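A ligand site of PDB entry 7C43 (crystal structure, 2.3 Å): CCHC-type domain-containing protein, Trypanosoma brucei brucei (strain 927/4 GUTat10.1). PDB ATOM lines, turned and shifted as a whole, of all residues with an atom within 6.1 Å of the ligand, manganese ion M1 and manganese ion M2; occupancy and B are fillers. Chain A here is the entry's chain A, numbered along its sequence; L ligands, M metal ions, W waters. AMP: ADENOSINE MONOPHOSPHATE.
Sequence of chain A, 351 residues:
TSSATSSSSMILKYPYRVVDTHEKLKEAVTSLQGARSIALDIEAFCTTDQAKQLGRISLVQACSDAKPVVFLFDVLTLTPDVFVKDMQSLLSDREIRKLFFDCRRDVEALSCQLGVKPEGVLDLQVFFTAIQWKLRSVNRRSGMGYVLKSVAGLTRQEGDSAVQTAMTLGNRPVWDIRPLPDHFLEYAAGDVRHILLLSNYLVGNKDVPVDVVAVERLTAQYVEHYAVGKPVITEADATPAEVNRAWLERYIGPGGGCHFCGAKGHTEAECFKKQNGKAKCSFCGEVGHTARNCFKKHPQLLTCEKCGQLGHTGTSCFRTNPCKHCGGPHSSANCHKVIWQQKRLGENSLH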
ATOM      1  N   LEU A  40     -11.821 -26.977  18.888  1.00  0.00           N
ATOM      2  CA  LEU A  40     -12.400 -25.890  19.659  1.00  0.00           C
ATOM      3  C   LEU A  40     -13.903 -25.812  19.579  1.00  0.00           C
ATOM      4  O   LEU A  40     -14.512 -26.295  18.641  1.00  0.00           O
ATOM      5  CB  LEU A  40     -11.842 -24.558  19.210  1.00  0.00           C
ATOM      6  CG  LEU A  40     -10.340 -24.413  19.393  1.00  0.00           C
ATOM      7  CD1 LEU A  40      -9.877 -23.142  18.706  1.00  0.00           C
ATOM      8  CD2 LEU A  40      -9.977 -24.418  20.878  1.00  0.00           C
ATOM      9  N   ASP A  41     -14.488 -25.221  20.612  1.00  0.00           N
ATOM     10  CA  ASP A  41     -15.886 -24.921  20.618  1.00  0.00           C
ATOM     11  C   ASP A  41     -16.111 -23.809  21.626  1.00  0.00           C
ATOM     12  O   ASP A  41     -15.245 -23.576  22.465  1.00  0.00           O
ATOM     13  CB  ASP A  41     -16.690 -26.163  21.005  1.00  0.00           C
ATOM     14  CG  ASP A  41     -18.174 -26.033  20.681  1.00  0.00           C
ATOM     15  OD1 ASP A  41     -18.541 -25.229  19.795  1.00  0.00           O
ATOM     16  OD2 ASP A  41     -18.955 -26.776  21.302  1.00  0.00           O
ATOM     17  N   ILE A  42     -17.274 -23.143  21.526  1.00  0.00           N
ATOM     18  CA  ILE A  42     -17.711 -22.116  22.492  1.00  0.00           C
ATOM     19  C   ILE A  42     -19.087 -22.434  23.084  1.00  0.00           C
ATOM     20  O   ILE A  42     -19.988 -22.775  22.350  1.00  0.00           O
ATOM     21  CB  ILE A  42     -17.771 -20.745  21.802  1.00  0.00           C
ATOM     22  CG1 ILE A  42     -16.376 -20.371  21.268  1.00  0.00           C
ATOM     23  CG2 ILE A  42     -18.307 -19.683  22.745  1.00  0.00           C
ATOM     24  CD1 ILE A  42     -16.288 -19.006  20.587  1.00  0.00           C
ATOM     25  N   GLU A  43     -19.231 -22.307  24.397  1.00  0.00           N
ATOM     26  CA  GLU A  43     -20.530 -22.264  25.035  1.00  0.00           C
ATOM     27  C   GLU A  43     -20.729 -20.827  25.415  1.00  0.00           C
ATOM     28  O   GLU A  43     -19.922 -20.273  26.153  1.00  0.00           O
ATOM     29  CB  GLU A  43     -20.619 -23.059  26.355  1.00  0.00           C
ATOM     30  CG  GLU A  43     -20.858 -24.553  26.350  1.00  0.00           C
ATOM     31  CD  GLU A  43     -21.720 -25.097  25.233  1.00  0.00           C
ATOM     32  OE1 GLU A  43     -21.313 -26.116  24.633  1.00  0.00           O
ATOM     33  OE2 GLU A  43     -22.783 -24.532  24.938  1.00  0.00           O
ATOM     34  N   ALA A  44     -21.876 -20.259  25.009  1.00  0.00           N
ATOM     35  CA  ALA A  44     -22.221 -18.874  25.252  1.00  0.00           C
ATOM     36  C   ALA A  44     -23.554 -18.754  25.996  1.00  0.00           C
ATOM     37  O   ALA A  44     -24.356 -19.693  25.994  1.00  0.00           O
ATOM     38  CB  ALA A  44     -22.305 -18.163  23.924  1.00  0.00           C
ATOM     39  N   PHE A  45     -23.770 -17.583  26.592  1.00  0.00           N
ATOM     40  CA  PHE A  45     -25.041 -17.237  27.210  1.00  0.00           C
ATOM     41  C   PHE A  45     -26.121 -17.293  26.144  1.00  0.00           C
ATOM     42  O   PHE A  45     -25.950 -16.743  25.075  1.00  0.00           O
ATOM     43  CB  PHE A  45     -25.029 -15.791  27.747  1.00  0.00           C
ATOM     44  CG  PHE A  45     -24.292 -15.579  29.027  1.00  0.00           C
ATOM     45  CD1 PHE A  45     -23.359 -16.509  29.527  1.00  0.00           C
ATOM     46  CD2 PHE A  45     -24.485 -14.396  29.720  1.00  0.00           C
ATOM     47  CE1 PHE A  45     -22.677 -16.269  30.711  1.00  0.00           C
ATOM     48  CE2 PHE A  45     -23.819 -14.153  30.911  1.00  0.00           C
ATOM     49  CZ  PHE A  45     -22.895 -15.082  31.405  1.00  0.00           C
ATOM     50  N   CYS A  46     -27.243 -17.913  26.463  1.00  0.00           N
ATOM     51  CA  CYS A  46     -28.341 -18.022  25.525  1.00  0.00           C
ATOM     52  C   CYS A  46     -28.948 -16.678  25.273  1.00  0.00           C
ATOM     53  O   CYS A  46     -29.117 -15.903  26.180  1.00  0.00           O
ATOM     54  CB  CYS A  46     -29.394 -18.971  26.062  1.00  0.00           C
ATOM     55  SG  CYS A  46     -28.808 -20.658  26.015  1.00  0.00           S
ATOM     56  N   THR A  47     -29.301 -16.400  24.053  1.00  0.00           N
ATOM     57  CA  THR A  47     -29.905 -15.142  23.760  1.00  0.00           C
ATOM     58  C   THR A  47     -31.408 -15.321  23.739  1.00  0.00           C
ATOM     59  O   THR A  47     -31.932 -16.184  23.075  1.00  0.00           O
ATOM     60  CB  THR A  47     -29.477 -14.623  22.396  1.00  0.00           C
ATOM     61  OG1 THR A  47     -30.021 -15.480  21.392  1.00  0.00           O
ATOM     62  CG2 THR A  47     -28.016 -14.662  22.252  1.00  0.00           C
ATOM     63  N   LEU A  54     -23.768 -15.275  18.889  1.00  0.00           N
ATOM     64  CA  LEU A  54     -23.651 -15.863  20.209  1.00  0.00           C
ATOM     65  C   LEU A  54     -23.710 -14.758  21.254  1.00  0.00           C
ATOM     66  O   LEU A  54     -23.204 -13.681  21.056  1.00  0.00           O
ATOM     67  CB  LEU A  54     -22.317 -16.601  20.381  1.00  0.00           C
ATOM     68  CG  LEU A  54     -22.007 -17.859  19.566  1.00  0.00           C
ATOM     69  CD1 LEU A  54     -20.703 -18.504  20.029  1.00  0.00           C
ATOM     70  CD2 LEU A  54     -23.147 -18.857  19.669  1.00  0.00           C
ATOM     71  N   GLY A  55     -24.329 -15.046  22.385  1.00  0.00           N
ATOM     72  CA  GLY A  55     -24.218 -14.192  23.561  1.00  0.00           C
ATOM     73  C   GLY A  55     -22.839 -14.268  24.191  1.00  0.00           C
ATOM     74  O   GLY A  55     -21.878 -14.714  23.589  1.00  0.00           O
ATOM     75  N   GLN A  61     -13.945 -24.535  24.941  1.00  0.00           N
ATOM     76  CA  GLN A  61     -13.616 -25.912  25.172  1.00  0.00           C
ATOM     77  C   GLN A  61     -12.529 -26.287  24.182  1.00  0.00           C
ATOM     78  O   GLN A  61     -12.631 -25.943  23.013  1.00  0.00           O
ATOM     79  CB  GLN A  61     -14.825 -26.791  24.867  1.00  0.00           C
ATOM     80  CG  GLN A  61     -16.041 -26.529  25.737  1.00  0.00           C
ATOM     81  CD  GLN A  61     -17.116 -25.703  25.066  1.00  0.00           C
ATOM     82  OE1 GLN A  61     -18.066 -26.221  24.503  1.00  0.00           O
ATOM     83  NE2 GLN A  61     -16.973 -24.394  25.146  1.00  0.00           N
ATOM     84  N   PHE A 101     -16.609 -27.445  14.312  1.00  0.00           N
ATOM     85  CA  PHE A 101     -17.834 -27.870  13.601  1.00  0.00           C
ATOM     86  C   PHE A 101     -18.853 -26.717  13.469  1.00  0.00           C
ATOM     87  O   PHE A 101     -19.558 -26.368  14.417  1.00  0.00           O
ATOM     88  CB  PHE A 101     -18.447 -29.091  14.290  1.00  0.00           C
ATOM     89  CG  PHE A 101     -19.468 -29.810  13.442  1.00  0.00           C
ATOM     90  CD1 PHE A 101     -20.816 -29.459  13.492  1.00  0.00           C
ATOM     91  CD2 PHE A 101     -19.077 -30.858  12.600  1.00  0.00           C
ATOM     92  CE1 PHE A 101     -21.762 -30.144  12.722  1.00  0.00           C
ATOM     93  CE2 PHE A 101     -20.018 -31.536  11.824  1.00  0.00           C
ATOM     94  CZ  PHE A 101     -21.362 -31.179  11.867  1.00  0.00           C
ATOM     95  N   ASP A 102     -18.941 -26.169  12.263  1.00  0.00           N
ATOM     96  CA  ASP A 102     -19.619 -24.879  11.980  1.00  0.00           C
ATOM     97  C   ASP A 102     -18.952 -23.757  12.734  1.00  0.00           C
ATOM     98  O   ASP A 102     -19.342 -23.462  13.851  1.00  0.00           O
ATOM     99  CB  ASP A 102     -21.128 -24.890  12.282  1.00  0.00           C
ATOM    100  CG  ASP A 102     -21.829 -23.650  11.764  1.00  0.00           C
ATOM    101  OD1 ASP A 102     -21.171 -22.747  11.201  1.00  0.00           O
ATOM    102  OD2 ASP A 102     -23.054 -23.551  11.906  1.00  0.00           O
ATOM    103  N   ASP A 106     -18.885 -18.941  16.019  1.00  0.00           N
ATOM    104  CA  ASP A 106     -17.767 -19.070  16.951  1.00  0.00           C
ATOM    105  C   ASP A 106     -16.686 -18.074  16.586  1.00  0.00           C
ATOM    106  O   ASP A 106     -16.129 -17.399  17.440  1.00  0.00           O
ATOM    107  CB  ASP A 106     -17.181 -20.493  16.921  1.00  0.00           C
ATOM    108  CG  ASP A 106     -18.097 -21.538  17.579  1.00  0.00           C
ATOM    109  OD1 ASP A 106     -19.018 -21.167  18.346  1.00  0.00           O
ATOM    110  OD2 ASP A 106     -17.880 -22.755  17.347  1.00  0.00           O
ATOM    111  N   GLN A 164     -30.170 -29.093  27.371  1.00  0.00           N
ATOM    112  CA  GLN A 164     -30.750 -28.792  26.081  1.00  0.00           C
ATOM    113  C   GLN A 164     -32.110 -28.104  26.200  1.00  0.00           C
ATOM    114  O   GLN A 164     -32.396 -27.224  25.390  1.00  0.00           O
ATOM    115  CB  GLN A 164     -30.873 -30.076  25.266  1.00  0.00           C
ATOM    116  CG  GLN A 164     -31.473 -29.886  23.891  1.00  0.00           C
ATOM    117  CD  GLN A 164     -31.512 -31.167  23.111  1.00  0.00           C
ATOM    118  OE1 GLN A 164     -31.260 -32.260  23.652  1.00  0.00           O
ATOM    119  NE2 GLN A 164     -31.821 -31.060  21.826  1.00  0.00           N
ATOM    120  N   MET A 167     -31.729 -24.417  27.421  1.00  0.00           N
ATOM    121  CA  MET A 167     -31.218 -23.657  26.293  1.00  0.00           C
ATOM    122  C   MET A 167     -32.313 -23.367  25.302  1.00  0.00           C
ATOM    123  O   MET A 167     -32.480 -22.221  24.901  1.00  0.00           O
ATOM    124  CB  MET A 167     -30.067 -24.380  25.579  1.00  0.00           C
ATOM    125  CG  MET A 167     -28.742 -24.325  26.338  1.00  0.00           C
ATOM    126  SD  MET A 167     -27.267 -24.891  25.132  1.00  0.00           S
ATOM    127  CE  MET A 167     -26.597 -26.226  26.370  1.00  0.00           C
ATOM    128  N   THR A 168     -33.070 -24.395  24.893  1.00  0.00           N
ATOM    129  CA  THR A 168     -34.104 -24.207  23.840  1.00  0.00           C
ATOM    130  C   THR A 168     -35.224 -23.242  24.275  1.00  0.00           C
ATOM    131  O   THR A 168     -35.788 -22.545  23.434  1.00  0.00           O
ATOM    132  CB  THR A 168     -34.712 -25.557  23.322  1.00  0.00           C
ATOM    133  OG1 THR A 168     -33.663 -26.482  23.023  1.00  0.00           O
ATOM    134  CG2 THR A 168     -35.554 -25.326  22.034  1.00  0.00           C
ATOM    135  N   LEU A 169     -35.533 -23.178  25.574  1.00  0.00           N
ATOM    136  CA  LEU A 169     -36.513 -22.210  26.071  1.00  0.00           C
ATOM    137  C   LEU A 169     -36.102 -20.742  25.784  1.00  0.00           C
ATOM    138  O   LEU A 169     -36.945 -19.923  25.402  1.00  0.00           O
ATOM    139  CB  LEU A 169     -36.833 -22.435  27.551  1.00  0.00           C
ATOM    140  CG  LEU A 169     -38.172 -21.846  28.044  1.00  0.00           C
ATOM    141  CD1 LEU A 169     -39.371 -22.276  27.199  1.00  0.00           C
ATOM    142  CD2 LEU A 169     -38.389 -22.214  29.502  1.00  0.00           C
ATOM    143  N   GLY A 170     -34.816 -20.425  25.949  1.00  0.00           N
ATOM    144  CA  GLY A 170     -34.234 -19.161  25.446  1.00  0.00           C
ATOM    145  C   GLY A 170     -34.548 -17.896  26.232  1.00  0.00           C
ATOM    146  O   GLY A 170     -34.272 -16.775  25.769  1.00  0.00           O
ATOM    147  N   TRP A 175     -25.709 -20.467  30.933  1.00  0.00           N
ATOM    148  CA  TRP A 175     -24.308 -20.658  31.094  1.00  0.00           C
ATOM    149  C   TRP A 175     -23.629 -19.693  32.004  1.00  0.00           C
ATOM    150  O   TRP A 175     -22.443 -19.719  32.123  1.00  0.00           O
ATOM    151  CB  TRP A 175     -23.660 -20.712  29.755  1.00  0.00           C
ATOM    152  CG  TRP A 175     -24.003 -21.936  29.014  1.00  0.00           C
ATOM    153  CD1 TRP A 175     -24.853 -22.045  27.988  1.00  0.00           C
ATOM    154  CD2 TRP A 175     -23.532 -23.248  29.261  1.00  0.00           C
ATOM    155  NE1 TRP A 175     -24.941 -23.308  27.569  1.00  0.00           N
ATOM    156  CE2 TRP A 175     -24.135 -24.081  28.335  1.00  0.00           C
ATOM    157  CE3 TRP A 175     -22.649 -23.795  30.178  1.00  0.00           C
ATOM    158  CZ2 TRP A 175     -23.892 -25.414  28.299  1.00  0.00           C
ATOM    159  CZ3 TRP A 175     -22.408 -25.106  30.130  1.00  0.00           C
ATOM    160  CH2 TRP A 175     -23.018 -25.903  29.205  1.00  0.00           C
ATOM    161  N   TYR A 187     -21.730 -31.825  29.324  1.00  0.00           N
ATOM    162  CA  TYR A 187     -22.396 -31.361  28.107  1.00  0.00           C
ATOM    163  C   TYR A 187     -21.442 -30.545  27.269  1.00  0.00           C
ATOM    164  O   TYR A 187     -21.342 -30.757  26.063  1.00  0.00           O
ATOM    165  CB  TYR A 187     -23.650 -30.514  28.410  1.00  0.00           C
ATOM    166  CG  TYR A 187     -24.535 -30.220  27.223  1.00  0.00           C
ATOM    167  CD1 TYR A 187     -24.155 -29.312  26.217  1.00  0.00           C
ATOM    168  CD2 TYR A 187     -25.779 -30.842  27.097  1.00  0.00           C
ATOM    169  CE1 TYR A 187     -24.994 -29.044  25.120  1.00  0.00           C
ATOM    170  CE2 TYR A 187     -26.625 -30.573  26.029  1.00  0.00           C
ATOM    171  CZ  TYR A 187     -26.221 -29.683  25.040  1.00  0.00           C
ATOM    172  OH  TYR A 187     -27.083 -29.447  23.990  1.00  0.00           O
ATOM    173  N   ALA A 188     -20.740 -29.614  27.912  1.00  0.00           N
ATOM    174  CA  ALA A 188     -19.787 -28.739  27.236  1.00  0.00           C
ATOM    175  C   ALA A 188     -18.638 -29.482  26.597  1.00  0.00           C
ATOM    176  O   ALA A 188     -18.193 -29.119  25.509  1.00  0.00           O
ATOM    177  CB  ALA A 188     -19.238 -27.712  28.193  1.00  0.00           C
ATOM    178  N   ASP A 191     -18.937 -31.834  22.442  1.00  0.00           N
ATOM    179  CA  ASP A 191     -18.660 -31.473  21.039  1.00  0.00           C
ATOM    180  C   ASP A 191     -17.186 -31.581  20.617  1.00  0.00           C
ATOM    181  O   ASP A 191     -16.905 -32.074  19.518  1.00  0.00           O
ATOM    182  CB  ASP A 191     -19.167 -30.065  20.718  1.00  0.00           C
ATOM    183  CG  ASP A 191     -20.703 -29.969  20.599  1.00  0.00           C
ATOM    184  OD1 ASP A 191     -21.368 -31.028  20.527  1.00  0.00           O
ATOM    185  OD2 ASP A 191     -21.221 -28.813  20.563  1.00  0.00           O
HETATM  186  P   AMP L   1     -23.038 -25.642  20.036  1.00  0.00           P
HETATM  187  O1P AMP L   1     -21.588 -25.724  20.385  1.00  0.00           O
HETATM  188  O2P AMP L   1     -23.603 -26.959  20.463  1.00  0.00           O
HETATM  189  O3P AMP L   1     -23.157 -25.235  18.607  1.00  0.00           O
HETATM  190  O5' AMP L   1     -23.687 -24.480  20.931  1.00  0.00           O
HETATM  191  C5' AMP L   1     -23.160 -23.132  20.888  1.00  0.00           C
HETATM  192  C4' AMP L   1     -23.988 -22.111  21.643  1.00  0.00           C
HETATM  193  O4' AMP L   1     -25.159 -21.737  20.880  1.00  0.00           O
HETATM  194  C3' AMP L   1     -24.528 -22.464  23.030  1.00  0.00           C
HETATM  195  O3' AMP L   1     -23.577 -22.320  24.074  1.00  0.00           O
HETATM  196  C2' AMP L   1     -25.666 -21.457  23.165  1.00  0.00           C
HETATM  197  O2' AMP L   1     -25.306 -20.125  23.471  1.00  0.00           O
HETATM  198  C1' AMP L   1     -26.248 -21.485  21.755  1.00  0.00           C
HETATM  199  N9  AMP L   1     -27.215 -22.567  21.589  1.00  0.00           N
HETATM  200  C8  AMP L   1     -26.945 -23.885  21.291  1.00  0.00           C
HETATM  201  N7  AMP L   1     -28.026 -24.636  21.239  1.00  0.00           N
HETATM  202  C5  AMP L   1     -29.058 -23.756  21.519  1.00  0.00           C
HETATM  203  C6  AMP L   1     -30.453 -23.941  21.608  1.00  0.00           C
HETATM  204  N6  AMP L   1     -31.050 -25.111  21.406  1.00  0.00           N
HETATM  205  N1  AMP L   1     -31.205 -22.864  21.902  1.00  0.00           N
HETATM  206  C2  AMP L   1     -30.596 -21.689  22.104  1.00  0.00           C
HETATM  207  N3  AMP L   1     -29.290 -21.391  22.048  1.00  0.00           N
HETATM  208  C4  AMP L   1     -28.570 -22.486  21.744  1.00  0.00           C
HETATM  209 MN    MN M   1     -21.124 -27.032  22.118  1.00  0.00          MN
HETATM  210 MN    MN M   2     -20.407 -25.076  18.767  1.00  0.00          MN
HETATM  211  O   HOH W   1     -19.658 -24.357  16.923  1.00  0.00           O
HETATM  212  O   HOH W   2     -20.215 -23.081  19.582  1.00  0.00           O
HETATM  213  O   HOH W   3     -25.620 -17.844  22.524  1.00  0.00           O
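The backbone NH (N) of Ala 44 lies within hydrogen-bond range of an oxygen (O3') of the ligand (2.8 Å). The side-chain hydroxyl (OG1) of Thr 168 lies within hydrogen-bond range of a nitrogen (N6) of the ligand, at 3.4 Å. The backbone carbonyl oxygen of Ala 44 is in hydrogen-bond range of an oxygen (O2') of the ligand (2.7 Å).
The indole nitrogen (NE1) of Trp 175 lies close to the side-chain sulfur (SD) of Met 167 (3.7 Å). NE2 of Gln 61 lies close to N of Glu 43 (3.2 Å). The side-chain amide oxygen (OE1) of Gln 61 lies close to the backbone carbonyl oxygen (O) of Ala 188 (3.1 Å). OG1 of Thr 168 sits at hydrogen-bond distance from O of Gln 164 (2.8 Å). The backbone carbonyl oxygen (O) of Asp 41 is in hydrogen-bond range of the backbone NH (N) of Gln 61 (3.0 Å).
N1 of the ligand sits close to O of Met 167 (3.3 Å). Residues that only touch the ligand: Ile 42, Leu 54, Phe 45 and Trp 175. Hydrophobic or aromatic side chains within 4 Å of the ligand: Ala 44, Leu 54 and Met 167. Within 4 Å of the ligand: Asp 41, Ile 42, Glu 43, Ala 44, Phe 45, Leu 54, Met 167, Thr 168, Trp 175 and Asp 191. The nearest printed residue that does not touch the ligand is Cys 46 (4.1 Å).
OE1 of Gln 61 touches manganese ion M1, 3.96 Å away.
Asp 106 touches manganese ion M2. Two residues have an atom within 4 Å of manganese ion M2: Asp 41 and Asp 106. The nearest printed residue that does not touch manganese ion M2 is Asp 191 (4.2 Å).
Manganese ion M1 is bound by O1P of the ligand, 2.2 Å away. OD2 of Asp 41 is bound to manganese ion M1 (2.3 Å). OD2 of Asp 191 is bound to manganese ion M1 (2.4 Å). The side-chain carboxylate (OE1) of Glu 43 is bound to manganese ion M1, at 2.7 Å. Manganese ion M1 has four donor atoms within binding distance.
Manganese ion M2 is bound by an oxygen (O1P) of the ligand, water W1, the side-chain carboxylate (OD1) of Asp 41 and water W2. Slightly farther from manganese ion M2 lies an oxygen (O3P) of the ligand (2.8 Å).
Water W2 lies within hydrogen-bond range of the side-chain carboxylate of Asp 106 (2.6 Å) and the backbone carbonyl oxygen of Ile 42 (2.8 Å). Water W3 lies within hydrogen-bond range of an oxygen (O2') of the ligand, the backbone carbonyl oxygen of Phe 45 and the backbone NH of Gly 55.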
